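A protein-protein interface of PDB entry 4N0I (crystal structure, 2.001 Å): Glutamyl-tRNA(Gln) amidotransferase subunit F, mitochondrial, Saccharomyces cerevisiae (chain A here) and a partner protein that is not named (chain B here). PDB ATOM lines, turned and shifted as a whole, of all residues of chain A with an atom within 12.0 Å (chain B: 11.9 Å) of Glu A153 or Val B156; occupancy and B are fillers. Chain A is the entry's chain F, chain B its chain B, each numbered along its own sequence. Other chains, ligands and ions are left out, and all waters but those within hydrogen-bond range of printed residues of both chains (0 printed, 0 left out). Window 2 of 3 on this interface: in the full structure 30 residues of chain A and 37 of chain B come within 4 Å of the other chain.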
ATOM      1  N   GLU A 143     -10.137  19.914  -7.557  1.00  0.00           N
ATOM      2  CA  GLU A 143     -10.773  21.152  -7.105  1.00  0.00           C
ATOM      3  C   GLU A 143     -12.237  20.905  -6.787  1.00  0.00           C
ATOM      4  O   GLU A 143     -12.876  20.015  -7.359  1.00  0.00           O
ATOM      5  CB  GLU A 143     -10.685  22.244  -8.176  1.00  0.00           C
ATOM      6  CG  GLU A 143      -9.298  22.464  -8.763  1.00  0.00           C
ATOM      7  CD  GLU A 143      -9.226  23.704  -9.635  1.00  0.00           C
ATOM      8  OE1 GLU A 143      -9.915  24.692  -9.312  1.00  0.00           O
ATOM      9  OE2 GLU A 143      -8.489  23.691 -10.647  1.00  0.00           O
ATOM     10  N   LYS A 145     -15.828  23.147  -4.609  1.00  0.00           N
ATOM     11  CA  LYS A 145     -16.279  24.257  -3.792  1.00  0.00           C
ATOM     12  C   LYS A 145     -17.248  23.677  -2.790  1.00  0.00           C
ATOM     13  O   LYS A 145     -18.360  23.278  -3.149  1.00  0.00           O
ATOM     14  CB  LYS A 145     -16.958  25.315  -4.646  1.00  0.00           C
ATOM     15  CG  LYS A 145     -17.604  26.414  -3.819  1.00  0.00           C
ATOM     16  CD  LYS A 145     -17.108  27.772  -4.236  1.00  0.00           C
ATOM     17  CE  LYS A 145     -17.731  28.871  -3.381  1.00  0.00           C
ATOM     18  NZ  LYS A 145     -17.440  30.177  -3.994  1.00  0.00           N
ATOM     19  N   PHE A 149     -18.815  19.835  -7.161  1.00  0.00           N
ATOM     20  CA  PHE A 149     -17.772  19.842  -8.181  1.00  0.00           C
ATOM     21  C   PHE A 149     -17.842  21.196  -8.874  1.00  0.00           C
ATOM     22  O   PHE A 149     -18.867  21.867  -8.816  1.00  0.00           O
ATOM     23  CB  PHE A 149     -17.976  18.726  -9.211  1.00  0.00           C
ATOM     24  CG  PHE A 149     -17.923  17.345  -8.625  1.00  0.00           C
ATOM     25  CD1 PHE A 149     -16.718  16.811  -8.184  1.00  0.00           C
ATOM     26  CD2 PHE A 149     -19.072  16.577  -8.521  1.00  0.00           C
ATOM     27  CE1 PHE A 149     -16.664  15.537  -7.647  1.00  0.00           C
ATOM     28  CE2 PHE A 149     -19.024  15.304  -7.980  1.00  0.00           C
ATOM     29  CZ  PHE A 149     -17.815  14.780  -7.547  1.00  0.00           C
ATOM     30  N   VAL A 150     -16.768  21.587  -9.543  1.00  0.00           N
ATOM     31  CA  VAL A 150     -16.723  22.889 -10.206  1.00  0.00           C
ATOM     32  C   VAL A 150     -16.213  22.790 -11.648  1.00  0.00           C
ATOM     33  O   VAL A 150     -15.347  21.966 -11.963  1.00  0.00           O
ATOM     34  CB  VAL A 150     -15.875  23.918  -9.404  1.00  0.00           C
ATOM     35  CG1 VAL A 150     -16.551  24.263  -8.092  1.00  0.00           C
ATOM     36  CG2 VAL A 150     -14.469  23.389  -9.147  1.00  0.00           C
ATOM     37  N   VAL A 151     -16.784  23.608 -12.526  1.00  0.00           N
ATOM     38  CA  VAL A 151     -16.301  23.725 -13.895  1.00  0.00           C
ATOM     39  C   VAL A 151     -16.134  25.205 -14.235  1.00  0.00           C
ATOM     40  O   VAL A 151     -16.995  26.024 -13.908  1.00  0.00           O
ATOM     41  CB  VAL A 151     -17.235  23.033 -14.918  1.00  0.00           C
ATOM     42  CG1 VAL A 151     -16.655  23.138 -16.325  1.00  0.00           C
ATOM     43  CG2 VAL A 151     -17.441  21.554 -14.562  1.00  0.00           C
ATOM     44  N   LYS A 152     -15.017  25.548 -14.867  1.00  0.00           N
ATOM     45  CA  LYS A 152     -14.707  26.937 -15.183  1.00  0.00           C
ATOM     46  C   LYS A 152     -15.204  27.334 -16.570  1.00  0.00           C
ATOM     47  O   LYS A 152     -14.873  26.694 -17.565  1.00  0.00           O
ATOM     48  CB  LYS A 152     -13.205  27.180 -15.075  1.00  0.00           C
ATOM     49  CG  LYS A 152     -12.594  26.723 -13.763  1.00  0.00           C
ATOM     50  CD  LYS A 152     -11.100  26.482 -13.925  1.00  0.00           C
ATOM     51  CE  LYS A 152     -10.482  25.905 -12.663  1.00  0.00           C
ATOM     52  NZ  LYS A 152      -9.033  25.613 -12.846  1.00  0.00           N
ATOM     53  N   GLU A 153     -15.997  28.400 -16.620  1.00  0.00           N
ATOM     54  CA  GLU A 153     -16.528  28.940 -17.871  1.00  0.00           C
ATOM     55  C   GLU A 153     -15.438  29.491 -18.794  1.00  0.00           C
ATOM     56  O   GLU A 153     -14.499  30.147 -18.344  1.00  0.00           O
ATOM     57  CB  GLU A 153     -17.556  30.039 -17.576  1.00  0.00           C
ATOM     58  N   TYR B  95     -20.197  17.395 -20.887  1.00  0.00           N
ATOM     59  CA  TYR B  95     -20.813  18.427 -20.078  1.00  0.00           C
ATOM     60  C   TYR B  95     -20.556  18.144 -18.609  1.00  0.00           C
ATOM     61  O   TYR B  95     -20.488  16.980 -18.195  1.00  0.00           O
ATOM     62  CB  TYR B  95     -22.319  18.498 -20.348  1.00  0.00           C
ATOM     63  CG  TYR B  95     -22.854  19.905 -20.446  1.00  0.00           C
ATOM     64  CD1 TYR B  95     -22.515  20.721 -21.520  1.00  0.00           C
ATOM     65  CD2 TYR B  95     -23.697  20.420 -19.468  1.00  0.00           C
ATOM     66  CE1 TYR B  95     -23.001  22.016 -21.617  1.00  0.00           C
ATOM     67  CE2 TYR B  95     -24.189  21.711 -19.556  1.00  0.00           C
ATOM     68  CZ  TYR B  95     -23.836  22.506 -20.633  1.00  0.00           C
ATOM     69  OH  TYR B  95     -24.322  23.794 -20.727  1.00  0.00           O
ATOM     70  N   GLY B  96     -20.458  19.215 -17.819  1.00  0.00           N
ATOM     71  CA  GLY B  96     -20.151  19.105 -16.407  1.00  0.00           C
ATOM     72  C   GLY B  96     -21.137  18.256 -15.629  1.00  0.00           C
ATOM     73  O   GLY B  96     -20.772  17.611 -14.644  1.00  0.00           O
ATOM     74  N   SER B 147     -26.789  21.976 -12.572  1.00  0.00           N
ATOM     75  CA  SER B 147     -25.759  23.007 -12.628  1.00  0.00           C
ATOM     76  C   SER B 147     -26.288  24.330 -12.098  1.00  0.00           C
ATOM     77  O   SER B 147     -27.408  24.731 -12.411  1.00  0.00           O
ATOM     78  CB  SER B 147     -25.262  23.199 -14.067  1.00  0.00           C
ATOM     79  OG  SER B 147     -24.654  22.026 -14.577  1.00  0.00           O
ATOM     80  N   HIS B 148     -25.486  24.972 -11.255  1.00  0.00           N
ATOM     81  CA  HIS B 148     -25.790  26.287 -10.706  1.00  0.00           C
ATOM     82  C   HIS B 148     -24.675  27.235 -11.127  1.00  0.00           C
ATOM     83  O   HIS B 148     -23.521  27.058 -10.737  1.00  0.00           O
ATOM     84  CB  HIS B 148     -25.897  26.231  -9.182  1.00  0.00           C
ATOM     85  CG  HIS B 148     -26.735  25.093  -8.684  1.00  0.00           C
ATOM     86  ND1 HIS B 148     -28.094  25.204  -8.477  1.00  0.00           N
ATOM     87  CD2 HIS B 148     -26.407  23.817  -8.370  1.00  0.00           C
ATOM     88  CE1 HIS B 148     -28.566  24.047  -8.048  1.00  0.00           C
ATOM     89  NE2 HIS B 148     -27.564  23.188  -7.971  1.00  0.00           N
ATOM     90  N   TYR B 149     -25.019  28.234 -11.933  1.00  0.00           N
ATOM     91  CA  TYR B 149     -24.033  29.175 -12.454  1.00  0.00           C
ATOM     92  C   TYR B 149     -23.837  30.360 -11.523  1.00  0.00           C
ATOM     93  O   TYR B 149     -24.784  31.077 -11.211  1.00  0.00           O
ATOM     94  CB  TYR B 149     -24.448  29.650 -13.849  1.00  0.00           C
ATOM     95  CG  TYR B 149     -24.693  28.518 -14.820  1.00  0.00           C
ATOM     96  CD1 TYR B 149     -23.662  28.012 -15.602  1.00  0.00           C
ATOM     97  CD2 TYR B 149     -25.955  27.947 -14.947  1.00  0.00           C
ATOM     98  CE1 TYR B 149     -23.881  26.970 -16.488  1.00  0.00           C
ATOM     99  CE2 TYR B 149     -26.182  26.905 -15.830  1.00  0.00           C
ATOM    100  CZ  TYR B 149     -25.144  26.421 -16.598  1.00  0.00           C
ATOM    101  OH  TYR B 149     -25.366  25.386 -17.478  1.00  0.00           O
ATOM    102  N   THR B 150     -22.604  30.542 -11.058  1.00  0.00           N
ATOM    103  CA  THR B 150     -22.277  31.635 -10.148  1.00  0.00           C
ATOM    104  C   THR B 150     -21.221  32.550 -10.760  1.00  0.00           C
ATOM    105  O   THR B 150     -20.022  32.293 -10.649  1.00  0.00           O
ATOM    106  CB  THR B 150     -21.756  31.112  -8.794  1.00  0.00           C
ATOM    107  OG1 THR B 150     -20.372  30.764  -8.910  1.00  0.00           O
ATOM    108  CG2 THR B 150     -22.550  29.899  -8.349  1.00  0.00           C
ATOM    109  N   VAL B 156     -16.035  33.348 -13.575  1.00  0.00           N
ATOM    110  CA  VAL B 156     -17.275  32.578 -13.534  1.00  0.00           C
ATOM    111  C   VAL B 156     -17.012  31.082 -13.338  1.00  0.00           C
ATOM    112  O   VAL B 156     -16.296  30.451 -14.121  1.00  0.00           O
ATOM    113  CB  VAL B 156     -18.128  32.792 -14.803  1.00  0.00           C
ATOM    114  CG1 VAL B 156     -19.587  32.468 -14.520  1.00  0.00           C
ATOM    115  CG2 VAL B 156     -17.989  34.209 -15.306  1.00  0.00           C
ATOM    116  N   ILE B 157     -17.621  30.510 -12.306  1.00  0.00           N
ATOM    117  CA  ILE B 157     -17.485  29.090 -12.041  1.00  0.00           C
ATOM    118  C   ILE B 157     -18.867  28.472 -11.900  1.00  0.00           C
ATOM    119  O   ILE B 157     -19.764  29.075 -11.310  1.00  0.00           O
ATOM    120  CB  ILE B 157     -16.616  28.837 -10.779  1.00  0.00           C
ATOM    121  CG1 ILE B 157     -15.163  28.566 -11.186  1.00  0.00           C
ATOM    122  CG2 ILE B 157     -17.162  27.691  -9.938  1.00  0.00           C
ATOM    123  CD1 ILE B 157     -14.260  28.134 -10.043  1.00  0.00           C
ATOM    124  N   THR B 158     -19.043  27.268 -12.435  1.00  0.00           N
ATOM    125  CA  THR B 158     -20.325  26.593 -12.320  1.00  0.00           C
ATOM    126  C   THR B 158     -20.222  25.420 -11.352  1.00  0.00           C
ATOM    127  O   THR B 158     -19.284  24.621 -11.407  1.00  0.00           O
ATOM    128  CB  THR B 158     -20.914  26.160 -13.689  1.00  0.00           C
ATOM    129  OG1 THR B 158     -21.103  24.739 -13.713  1.00  0.00           O
ATOM    130  CG2 THR B 158     -20.016  26.583 -14.829  1.00  0.00           C
ATOM    131  N   LEU B 159     -21.193  25.353 -10.449  1.00  0.00           N
ATOM    132  CA  LEU B 159     -21.230  24.349  -9.399  1.00  0.00           C
ATOM    133  C   LEU B 159     -22.065  23.173  -9.877  1.00  0.00           C
ATOM    134  O   LEU B 159     -23.149  23.363 -10.422  1.00  0.00           O
ATOM    135  CB  LEU B 159     -21.823  24.939  -8.114  1.00  0.00           C
ATOM    136  CG  LEU B 159     -21.110  26.182  -7.575  1.00  0.00           C
ATOM    137  CD1 LEU B 159     -21.904  26.809  -6.441  1.00  0.00           C
ATOM    138  CD2 LEU B 159     -19.702  25.844  -7.116  1.00  0.00           C
ATOM    139  N   VAL B 160     -21.547  21.961  -9.691  1.00  0.00           N
ATOM    140  CA  VAL B 160     -22.211  20.765 -10.190  1.00  0.00           C
ATOM    141  C   VAL B 160     -22.611  19.854  -9.038  1.00  0.00           C
ATOM    142  O   VAL B 160     -21.783  19.464  -8.215  1.00  0.00           O
ATOM    143  CB  VAL B 160     -21.323  19.973 -11.188  1.00  0.00           C
ATOM    144  CG1 VAL B 160     -22.069  18.749 -11.704  1.00  0.00           C
ATOM    145  CG2 VAL B 160     -20.886  20.853 -12.345  1.00  0.00           C
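The backbone carbonyl oxygen of His B148 lies within hydrogen-bond range of the backbone NH of Leu B159, at 2.9 Å. OG1 of Thr B150 sits at hydrogen-bond distance from O of Ile B157 (3.0 Å).
Among the printed residues, merely in contact across the chains: Val A150 with Thr B158 (3.3 Å), Phe A149 with Leu B159 (3.5 Å), Val A151 with Ile B157 (3.6 Å), Val A150 with Leu B159 (3.7 Å), Lys A145 with Leu B159 (3.7 Å), Phe A149 with Thr B158 (3.8 Å) and Val A150 with Ile B157 (3.9 Å).
O of Val B156 sits at hydrogen-bond distance from N of Glu A153 (3.2 Å). N of Thr B158 is in hydrogen-bond range of O of Val A151 (2.8 Å). N of Val B160 is in hydrogen-bond range of O of Phe A149 (2.8 Å).
Of chain B, only Val B156 (3.2 Å) comes within 4 Å of Glu A153. Val A151 touches just these residues of chain B: Ile B157 and Thr B158. Ile B157 touches just these residues of chain A: Val A150 (3.9 Å) and Val A151 (3.6 Å). Of chain A, only Phe A149 (3.8 Å), Val A150 (3.3 Å) and Val A151 (2.8 Å) come within 4 Å of Thr B158. Of the printed residues of chain B, Phe A149 touches Thr B158, Leu B159 and Val B160. Printed residues of chain A within 4 Å of Leu B159: Lys A145 (3.7 Å), Phe A149 (3.5 Å) and Val A150 (3.7 Å). Of the printed residues of chain B, Lys A145 touches Leu B159 (3.7 Å). Gly B96 touches none of the printed residues of chain A. The nearest residue of chain B that does not touch Glu A153 is Thr B158 (4.8 Å). The nearest printed residue of chain B that does not touch Phe A149 is Ile B157 (6.2 Å).
Hydrophobic or aromatic side chains of chain A that line the printed part of chain B: Phe A149 and Val A150. Along chain A the printed residues that touch a printed residue of chain B span positions 145 to 153.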
